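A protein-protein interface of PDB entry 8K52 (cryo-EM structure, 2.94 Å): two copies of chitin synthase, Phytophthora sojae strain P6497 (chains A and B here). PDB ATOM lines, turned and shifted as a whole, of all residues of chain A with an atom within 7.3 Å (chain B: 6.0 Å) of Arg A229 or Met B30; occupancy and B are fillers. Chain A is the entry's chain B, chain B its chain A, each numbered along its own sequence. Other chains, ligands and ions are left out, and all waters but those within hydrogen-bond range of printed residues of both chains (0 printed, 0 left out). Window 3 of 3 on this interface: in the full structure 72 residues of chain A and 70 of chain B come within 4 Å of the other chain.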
ATOM      1  N   ARG A 220      12.151 -34.079 -22.850  1.00  0.00           N
ATOM      2  CA  ARG A 220      12.272 -32.830 -22.119  1.00  0.00           C
ATOM      3  C   ARG A 220      11.868 -33.054 -20.672  1.00  0.00           C
ATOM      4  O   ARG A 220      11.052 -33.926 -20.363  1.00  0.00           O
ATOM      5  CB  ARG A 220      11.422 -31.718 -22.744  1.00  0.00           C
ATOM      6  CG  ARG A 220      11.567 -31.631 -24.247  1.00  0.00           C
ATOM      7  CD  ARG A 220      12.936 -31.084 -24.614  1.00  0.00           C
ATOM      8  NE  ARG A 220      13.316 -31.428 -25.978  1.00  0.00           N
ATOM      9  CZ  ARG A 220      14.357 -30.913 -26.616  1.00  0.00           C
ATOM     10  NH1 ARG A 220      15.140 -30.013 -26.044  1.00  0.00           N
ATOM     11  NH2 ARG A 220      14.619 -31.308 -27.857  1.00  0.00           N
ATOM     12  N   CYS A 223      11.803 -29.037 -15.666  1.00  0.00           N
ATOM     13  CA  CYS A 223      12.603 -27.824 -15.553  1.00  0.00           C
ATOM     14  C   CYS A 223      12.753 -27.140 -16.904  1.00  0.00           C
ATOM     15  O   CYS A 223      12.575 -25.920 -17.015  1.00  0.00           O
ATOM     16  CB  CYS A 223      13.971 -28.165 -14.968  1.00  0.00           C
ATOM     17  SG  CYS A 223      13.885 -29.201 -13.495  1.00  0.00           S
ATOM     18  N   VAL A 224      13.053 -27.913 -17.948  1.00  0.00           N
ATOM     19  CA  VAL A 224      13.197 -27.339 -19.282  1.00  0.00           C
ATOM     20  C   VAL A 224      11.871 -26.766 -19.764  1.00  0.00           C
ATOM     21  O   VAL A 224      11.822 -25.669 -20.333  1.00  0.00           O
ATOM     22  CB  VAL A 224      13.746 -28.394 -20.258  1.00  0.00           C
ATOM     23  CG1 VAL A 224      14.163 -27.738 -21.562  1.00  0.00           C
ATOM     24  CG2 VAL A 224      14.907 -29.142 -19.629  1.00  0.00           C
ATOM     25  N   THR A 226       9.237 -25.667 -18.033  1.00  0.00           N
ATOM     26  CA  THR A 226       8.888 -24.452 -17.313  1.00  0.00           C
ATOM     27  C   THR A 226       9.940 -23.360 -17.450  1.00  0.00           C
ATOM     28  O   THR A 226       9.710 -22.239 -16.983  1.00  0.00           O
ATOM     29  CB  THR A 226       8.659 -24.759 -15.831  1.00  0.00           C
ATOM     30  OG1 THR A 226       9.885 -25.203 -15.238  1.00  0.00           O
ATOM     31  CG2 THR A 226       7.591 -25.829 -15.664  1.00  0.00           C
ATOM     32  N   GLY A 227      11.078 -23.654 -18.074  1.00  0.00           N
ATOM     33  CA  GLY A 227      12.104 -22.657 -18.273  1.00  0.00           C
ATOM     34  C   GLY A 227      13.100 -22.543 -17.147  1.00  0.00           C
ATOM     35  O   GLY A 227      14.034 -21.737 -17.247  1.00  0.00           O
ATOM     36  N   ARG A 228      12.931 -23.312 -16.076  1.00  0.00           N
ATOM     37  CA  ARG A 228      13.896 -23.300 -14.988  1.00  0.00           C
ATOM     38  C   ARG A 228      15.227 -23.857 -15.468  1.00  0.00           C
ATOM     39  O   ARG A 228      15.280 -24.860 -16.184  1.00  0.00           O
ATOM     40  CB  ARG A 228      13.372 -24.108 -13.805  1.00  0.00           C
ATOM     41  CG  ARG A 228      12.042 -23.603 -13.283  1.00  0.00           C
ATOM     42  CD  ARG A 228      11.512 -24.471 -12.163  1.00  0.00           C
ATOM     43  NE  ARG A 228      10.230 -23.976 -11.675  1.00  0.00           N
ATOM     44  CZ  ARG A 228       9.495 -24.581 -10.754  1.00  0.00           C
ATOM     45  NH1 ARG A 228       9.893 -25.706 -10.182  1.00  0.00           N
ATOM     46  NH2 ARG A 228       8.337 -24.039 -10.389  1.00  0.00           N
ATOM     47  N   ARG A 229      16.309 -23.194 -15.068  1.00  0.00           N
ATOM     48  CA  ARG A 229      17.654 -23.526 -15.528  1.00  0.00           C
ATOM     49  C   ARG A 229      18.459 -23.959 -14.312  1.00  0.00           C
ATOM     50  O   ARG A 229      19.079 -23.127 -13.636  1.00  0.00           O
ATOM     51  CB  ARG A 229      18.304 -22.335 -16.227  1.00  0.00           C
ATOM     52  CG  ARG A 229      18.910 -22.659 -17.576  1.00  0.00           C
ATOM     53  CD  ARG A 229      17.821 -22.904 -18.606  1.00  0.00           C
ATOM     54  NE  ARG A 229      16.991 -21.731 -18.861  1.00  0.00           N
ATOM     55  CZ  ARG A 229      17.421 -20.598 -19.401  1.00  0.00           C
ATOM     56  NH1 ARG A 229      18.675 -20.446 -19.793  1.00  0.00           N
ATOM     57  NH2 ARG A 229      16.565 -19.593 -19.563  1.00  0.00           N
ATOM     58  N   PRO A 230      18.462 -25.251 -13.995  1.00  0.00           N
ATOM     59  CA  PRO A 230      19.231 -25.721 -12.841  1.00  0.00           C
ATOM     60  C   PRO A 230      20.720 -25.496 -13.034  1.00  0.00           C
ATOM     61  O   PRO A 230      21.258 -25.627 -14.136  1.00  0.00           O
ATOM     62  CB  PRO A 230      18.896 -27.215 -12.773  1.00  0.00           C
ATOM     63  CG  PRO A 230      18.465 -27.569 -14.148  1.00  0.00           C
ATOM     64  CD  PRO A 230      17.780 -26.353 -14.693  1.00  0.00           C
ATOM     65  N   ARG A 231      21.387 -25.148 -11.937  1.00  0.00           N
ATOM     66  CA  ARG A 231      22.822 -24.910 -11.944  1.00  0.00           C
ATOM     67  C   ARG A 231      23.609 -25.971 -11.198  1.00  0.00           C
ATOM     68  O   ARG A 231      24.537 -26.548 -11.768  1.00  0.00           O
ATOM     69  CB  ARG A 231      23.135 -23.539 -11.334  1.00  0.00           C
ATOM     70  CG  ARG A 231      23.091 -22.366 -12.312  1.00  0.00           C
ATOM     71  CD  ARG A 231      23.752 -22.683 -13.645  1.00  0.00           C
ATOM     72  NE  ARG A 231      22.818 -23.237 -14.619  1.00  0.00           N
ATOM     73  CZ  ARG A 231      23.180 -23.828 -15.749  1.00  0.00           C
ATOM     74  NH1 ARG A 231      24.453 -23.957 -16.084  1.00  0.00           N
ATOM     75  NH2 ARG A 231      22.242 -24.303 -16.562  1.00  0.00           N
ATOM     76  N   LEU A 232      23.257 -26.248  -9.948  1.00  0.00           N
ATOM     77  CA  LEU A 232      23.824 -27.355  -9.197  1.00  0.00           C
ATOM     78  C   LEU A 232      22.960 -28.581  -9.443  1.00  0.00           C
ATOM     79  O   LEU A 232      21.729 -28.495  -9.437  1.00  0.00           O
ATOM     80  CB  LEU A 232      23.895 -27.033  -7.699  1.00  0.00           C
ATOM     81  CG  LEU A 232      24.464 -28.053  -6.704  1.00  0.00           C
ATOM     82  CD1 LEU A 232      23.411 -29.034  -6.207  1.00  0.00           C
ATOM     83  CD2 LEU A 232      25.654 -28.796  -7.293  1.00  0.00           C
ATOM     84  N   ALA A 274      23.304 -16.837  -7.990  1.00  0.00           N
ATOM     85  CA  ALA A 274      22.158 -17.706  -8.228  1.00  0.00           C
ATOM     86  C   ALA A 274      21.791 -18.562  -7.026  1.00  0.00           C
ATOM     87  O   ALA A 274      20.744 -19.217  -7.055  1.00  0.00           O
ATOM     88  CB  ALA A 274      22.430 -18.604  -9.434  1.00  0.00           C
ATOM     89  N   GLN A 282      14.874 -23.684  -6.387  1.00  0.00           N
ATOM     90  CA  GLN A 282      14.549 -23.656  -7.808  1.00  0.00           C
ATOM     91  C   GLN A 282      15.744 -24.048  -8.664  1.00  0.00           C
ATOM     92  O   GLN A 282      15.577 -24.690  -9.706  1.00  0.00           O
ATOM     93  CB  GLN A 282      14.063 -22.260  -8.204  1.00  0.00           C
ATOM     94  CG  GLN A 282      12.675 -21.897  -7.706  1.00  0.00           C
ATOM     95  CD  GLN A 282      11.573 -22.474  -8.562  1.00  0.00           C
ATOM     96  OE1 GLN A 282      11.722 -23.543  -9.147  1.00  0.00           O
ATOM     97  NE2 GLN A 282      10.453 -21.765  -8.640  1.00  0.00           N
ATOM     98  N   ASN A 283      16.948 -23.679  -8.239  1.00  0.00           N
ATOM     99  CA  ASN A 283      18.149 -23.779  -9.052  1.00  0.00           C
ATOM    100  C   ASN A 283      18.891 -25.098  -8.877  1.00  0.00           C
ATOM    101  O   ASN A 283      19.928 -25.296  -9.516  1.00  0.00           O
ATOM    102  CB  ASN A 283      19.081 -22.609  -8.723  1.00  0.00           C
ATOM    103  CG  ASN A 283      20.095 -22.346  -9.810  1.00  0.00           C
ATOM    104  OD1 ASN A 283      19.924 -22.775 -10.949  1.00  0.00           O
ATOM    105  ND2 ASN A 283      21.158 -21.634  -9.464  1.00  0.00           N
ATOM    106  N   VAL A 284      18.395 -26.001  -8.036  1.00  0.00           N
ATOM    107  CA  VAL A 284      19.065 -27.263  -7.748  1.00  0.00           C
ATOM    108  C   VAL A 284      18.139 -28.410  -8.119  1.00  0.00           C
ATOM    109  O   VAL A 284      16.976 -28.439  -7.703  1.00  0.00           O
ATOM    110  CB  VAL A 284      19.479 -27.358  -6.265  1.00  0.00           C
ATOM    111  CG1 VAL A 284      19.765 -28.801  -5.882  1.00  0.00           C
ATOM    112  CG2 VAL A 284      20.681 -26.473  -5.991  1.00  0.00           C
ATOM    113  N   GLN A 346      13.450 -30.261  -6.014  1.00  0.00           N
ATOM    114  CA  GLN A 346      13.227 -30.711  -7.384  1.00  0.00           C
ATOM    115  C   GLN A 346      13.936 -32.044  -7.580  1.00  0.00           C
ATOM    116  O   GLN A 346      15.166 -32.115  -7.499  1.00  0.00           O
ATOM    117  CB  GLN A 346      13.738 -29.663  -8.368  1.00  0.00           C
ATOM    118  CG  GLN A 346      12.877 -29.470  -9.599  1.00  0.00           C
ATOM    119  CD  GLN A 346      13.065 -28.104 -10.229  1.00  0.00           C
ATOM    120  OE1 GLN A 346      12.124 -27.520 -10.764  1.00  0.00           O
ATOM    121  NE2 GLN A 346      14.285 -27.584 -10.163  1.00  0.00           N
ATOM    122  N   GLN A 372      21.475 -32.617 -21.296  1.00  0.00           N
ATOM    123  CA  GLN A 372      20.212 -31.927 -21.516  1.00  0.00           C
ATOM    124  C   GLN A 372      20.203 -30.543 -20.878  1.00  0.00           C
ATOM    125  O   GLN A 372      19.940 -29.545 -21.556  1.00  0.00           O
ATOM    126  CB  GLN A 372      19.054 -32.764 -20.979  1.00  0.00           C
ATOM    127  CG  GLN A 372      17.701 -32.166 -21.288  1.00  0.00           C
ATOM    128  CD  GLN A 372      16.719 -33.191 -21.788  1.00  0.00           C
ATOM    129  OE1 GLN A 372      17.095 -34.305 -22.144  1.00  0.00           O
ATOM    130  NE2 GLN A 372      15.449 -32.821 -21.823  1.00  0.00           N
ATOM    131  N   ILE A 373      20.490 -30.458 -19.579  1.00  0.00           N
ATOM    132  CA  ILE A 373      20.254 -29.199 -18.871  1.00  0.00           C
ATOM    133  C   ILE A 373      21.512 -28.376 -18.611  1.00  0.00           C
ATOM    134  O   ILE A 373      21.397 -27.219 -18.179  1.00  0.00           O
ATOM    135  CB  ILE A 373      19.514 -29.432 -17.542  1.00  0.00           C
ATOM    136  CG1 ILE A 373      20.187 -30.524 -16.721  1.00  0.00           C
ATOM    137  CG2 ILE A 373      18.057 -29.780 -17.800  1.00  0.00           C
ATOM    138  CD1 ILE A 373      19.317 -31.044 -15.606  1.00  0.00           C
ATOM    139  N   GLN A 374      22.701 -28.926 -18.861  1.00  0.00           N
ATOM    140  CA  GLN A 374      23.971 -28.217 -18.753  1.00  0.00           C
ATOM    141  C   GLN A 374      24.143 -27.574 -17.382  1.00  0.00           C
ATOM    142  O   GLN A 374      24.103 -26.344 -17.265  1.00  0.00           O
ATOM    143  CB  GLN A 374      24.088 -27.158 -19.849  1.00  0.00           C
ATOM    144  CG  GLN A 374      24.431 -27.707 -21.230  1.00  0.00           C
ATOM    145  CD  GLN A 374      25.605 -28.672 -21.227  1.00  0.00           C
ATOM    146  OE1 GLN A 374      26.509 -28.577 -20.397  1.00  0.00           O
ATOM    147  NE2 GLN A 374      25.594 -29.608 -22.166  1.00  0.00           N
ATOM    148  N   PRO A 375      24.332 -28.362 -16.329  1.00  0.00           N
ATOM    149  CA  PRO A 375      24.525 -27.779 -15.001  1.00  0.00           C
ATOM    150  C   PRO A 375      25.879 -27.099 -14.883  1.00  0.00           C
ATOM    151  O   PRO A 375      26.833 -27.418 -15.593  1.00  0.00           O
ATOM    152  CB  PRO A 375      24.430 -28.989 -14.072  1.00  0.00           C
ATOM    153  CG  PRO A 375      24.935 -30.112 -14.899  1.00  0.00           C
ATOM    154  CD  PRO A 375      24.511 -29.824 -16.317  1.00  0.00           C
ATOM    155  N   PRO B  25      26.020 -17.851 -23.916  1.00  0.00           N
ATOM    156  CA  PRO B  25      25.925 -19.235 -24.414  1.00  0.00           C
ATOM    157  C   PRO B  25      24.723 -19.988 -23.874  1.00  0.00           C
ATOM    158  O   PRO B  25      24.105 -20.769 -24.610  1.00  0.00           O
ATOM    159  CB  PRO B  25      27.246 -19.865 -23.952  1.00  0.00           C
ATOM    160  CG  PRO B  25      28.166 -18.717 -23.757  1.00  0.00           C
ATOM    161  CD  PRO B  25      27.307 -17.613 -23.238  1.00  0.00           C
ATOM    162  N   ARG B  26      24.368 -19.769 -22.605  1.00  0.00           N
ATOM    163  CA  ARG B  26      23.193 -20.432 -22.045  1.00  0.00           C
ATOM    164  C   ARG B  26      21.935 -20.014 -22.789  1.00  0.00           C
ATOM    165  O   ARG B  26      21.106 -20.857 -23.157  1.00  0.00           O
ATOM    166  CB  ARG B  26      23.060 -20.094 -20.561  1.00  0.00           C
ATOM    167  CG  ARG B  26      23.960 -20.843 -19.555  1.00  0.00           C
ATOM    168  CD  ARG B  26      23.638 -22.337 -19.305  1.00  0.00           C
ATOM    169  NE  ARG B  26      23.462 -23.231 -20.449  1.00  0.00           N
ATOM    170  CZ  ARG B  26      24.290 -23.345 -21.483  1.00  0.00           C
ATOM    171  NH1 ARG B  26      25.425 -22.666 -21.547  1.00  0.00           N
ATOM    172  NH2 ARG B  26      23.990 -24.188 -22.464  1.00  0.00           N
ATOM    173  N   SER B  27      21.788 -18.710 -23.030  1.00  0.00           N
ATOM    174  CA  SER B  27      20.619 -18.205 -23.735  1.00  0.00           C
ATOM    175  C   SER B  27      20.579 -18.721 -25.167  1.00  0.00           C
ATOM    176  O   SER B  27      19.510 -19.075 -25.676  1.00  0.00           O
ATOM    177  CB  SER B  27      20.615 -16.677 -23.705  1.00  0.00           C
ATOM    178  OG  SER B  27      21.130 -16.199 -22.473  1.00  0.00           O
ATOM    179  N   SER B  28      21.736 -18.776 -25.834  1.00  0.00           N
ATOM    180  CA  SER B  28      21.776 -19.287 -27.200  1.00  0.00           C
ATOM    181  C   SER B  28      21.379 -20.757 -27.254  1.00  0.00           C
ATOM    182  O   SER B  28      20.605 -21.168 -28.129  1.00  0.00           O
ATOM    183  CB  SER B  28      23.170 -19.093 -27.796  1.00  0.00           C
ATOM    184  OG  SER B  28      23.226 -19.578 -29.126  1.00  0.00           O
ATOM    185  N   MET B  29      21.893 -21.563 -26.321  1.00  0.00           N
ATOM    186  CA  MET B  29      21.560 -22.982 -26.324  1.00  0.00           C
ATOM    187  C   MET B  29      20.084 -23.198 -26.021  1.00  0.00           C
ATOM    188  O   MET B  29      19.426 -24.032 -26.653  1.00  0.00           O
ATOM    189  CB  MET B  29      22.431 -23.732 -25.319  1.00  0.00           C
ATOM    190  CG  MET B  29      21.784 -24.986 -24.759  1.00  0.00           C
ATOM    191  SD  MET B  29      23.016 -26.195 -24.245  1.00  0.00           S
ATOM    192  CE  MET B  29      21.976 -27.610 -23.903  1.00  0.00           C
ATOM    193  N   MET B  30      19.535 -22.445 -25.068  1.00  0.00           N
ATOM    194  CA  MET B  30      18.117 -22.608 -24.773  1.00  0.00           C
ATOM    195  C   MET B  30      17.243 -22.094 -25.912  1.00  0.00           C
ATOM    196  O   MET B  30      16.160 -22.633 -26.143  1.00  0.00           O
ATOM    197  CB  MET B  30      17.769 -21.927 -23.451  1.00  0.00           C
ATOM    198  CG  MET B  30      18.258 -22.721 -22.251  1.00  0.00           C
ATOM    199  SD  MET B  30      18.407 -24.473 -22.668  1.00  0.00           S
ATOM    200  CE  MET B  30      18.757 -25.207 -21.074  1.00  0.00           C
ATOM    201  N   SER B  31      17.701 -21.080 -26.650  1.00  0.00           N
ATOM    202  CA  SER B  31      16.952 -20.619 -27.815  1.00  0.00           C
ATOM    203  C   SER B  31      16.943 -21.671 -28.919  1.00  0.00           C
ATOM    204  O   SER B  31      15.902 -21.913 -29.546  1.00  0.00           O
ATOM    205  CB  SER B  31      17.534 -19.303 -28.327  1.00  0.00           C
ATOM    206  OG  SER B  31      17.515 -18.309 -27.317  1.00  0.00           O
ATOM    207  N   VAL B  32      18.091 -22.305 -29.180  1.00  0.00           N
ATOM    208  CA  VAL B  32      18.093 -23.360 -30.190  1.00  0.00           C
ATOM    209  C   VAL B  32      17.267 -24.552 -29.719  1.00  0.00           C
ATOM    210  O   VAL B  32      16.598 -25.203 -30.526  1.00  0.00           O
ATOM    211  CB  VAL B  32      19.526 -23.767 -30.597  1.00  0.00           C
ATOM    212  CG1 VAL B  32      20.366 -22.535 -30.905  1.00  0.00           C
ATOM    213  CG2 VAL B  32      20.190 -24.626 -29.536  1.00  0.00           C
ATOM    214  N   GLU B  33      17.256 -24.839 -28.415  1.00  0.00           N
ATOM    215  CA  GLU B  33      16.362 -25.879 -27.910  1.00  0.00           C
ATOM    216  C   GLU B  33      14.901 -25.508 -28.151  1.00  0.00           C
ATOM    217  O   GLU B  33      14.113 -26.325 -28.646  1.00  0.00           O
ATOM    218  CB  GLU B  33      16.621 -26.115 -26.422  1.00  0.00           C
ATOM    219  CG  GLU B  33      17.918 -26.846 -26.128  1.00  0.00           C
ATOM    220  CD  GLU B  33      17.699 -28.304 -25.777  1.00  0.00           C
ATOM    221  OE1 GLU B  33      17.150 -28.581 -24.691  1.00  0.00           O
ATOM    222  OE2 GLU B  33      18.073 -29.173 -26.590  1.00  0.00           O
ATOM    223  N   TYR B  34      14.540 -24.260 -27.831  1.00  0.00           N
ATOM    224  CA  TYR B  34      13.175 -23.774 -28.016  1.00  0.00           C
ATOM    225  C   TYR B  34      12.742 -23.901 -29.467  1.00  0.00           C
ATOM    226  O   TYR B  34      11.592 -24.259 -29.751  1.00  0.00           O
ATOM    227  CB  TYR B  34      13.074 -22.321 -27.545  1.00  0.00           C
ATOM    228  CG  TYR B  34      11.713 -21.687 -27.736  1.00  0.00           C
ATOM    229  CD1 TYR B  34      10.706 -21.857 -26.795  1.00  0.00           C
ATOM    230  CD2 TYR B  34      11.439 -20.904 -28.853  1.00  0.00           C
ATOM    231  CE1 TYR B  34       9.463 -21.275 -26.963  1.00  0.00           C
ATOM    232  CE2 TYR B  34      10.200 -20.319 -29.029  1.00  0.00           C
ATOM    233  CZ  TYR B  34       9.216 -20.508 -28.081  1.00  0.00           C
ATOM    234  OH  TYR B  34       7.980 -19.927 -28.253  1.00  0.00           O
ATOM    235  N   ASP B  35      13.642 -23.596 -30.399  1.00  0.00           N
ATOM    236  CA  ASP B  35      13.389 -23.933 -31.793  1.00  0.00           C
ATOM    237  C   ASP B  35      13.334 -25.441 -32.007  1.00  0.00           C
ATOM    238  O   ASP B  35      12.706 -25.901 -32.966  1.00  0.00           O
ATOM    239  CB  ASP B  35      14.459 -23.312 -32.692  1.00  0.00           C
ATOM    240  CG  ASP B  35      13.997 -23.158 -34.128  1.00  0.00           C
ATOM    241  OD1 ASP B  35      12.788 -23.338 -34.386  1.00  0.00           O
ATOM    242  OD2 ASP B  35      14.840 -22.853 -34.997  1.00  0.00           O
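NH1 of Arg A220 is in salt-bridge range of OE1 of Glu B33 (2.8 Å).
No position is printed for both chains.
Met B30 touches Arg A229. CD of Arg B26 touches NH2 of Arg A231, at 3.7 Å. Gln A372 touches Met B29. Arg B26 touches Gln A374 (NH2 to CG, 3.8 Å). Met B29 touches Gln A374.
Of the printed residues of chain B, Arg A220 touches Glu B33 (2.8 Å). Gly A227 touches none of the printed residues of chain B. Of chain B, only Met B30 (3.4 Å) comes within 4 Å of Arg A229. Of the printed residues of chain B, Arg A231 touches Arg B26 (3.7 Å). Of the printed residues of chain A, Arg B26 touches Arg A231 (3.7 Å) and Gln A374 (3.8 Å). Met B30 touches just one residue of chain A: Arg A229. The nearest residue of chain B that does not touch Arg A229 is Arg B26 (4.2 Å).
The backbone carbonyl oxygen (O) of Gly A227 is in hydrogen-bond range of the guanidinium group (NE) of Arg A229. The guanidinium group (NH2) of Arg B26 lies within hydrogen-bond range of the side-chain sulfur (SD) of Met B29, at 2.9 Å. NH1 of Arg A231 is in hydrogen-bond range of O of Gln A374, at 2.7 Å. The backbone NH of Arg A231 lies within hydrogen-bond range of the backbone carbonyl oxygen of Asn A283, 2.8 Å away. The backbone carbonyl oxygen (O) of Arg A229 sits close to the side-chain amide oxygen (OD1) of Asn A283 (2.8 Å). The guanidinium group of Arg A231 lies within hydrogen-bond range of the backbone carbonyl oxygen of Ile A373 (3.4 Å).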
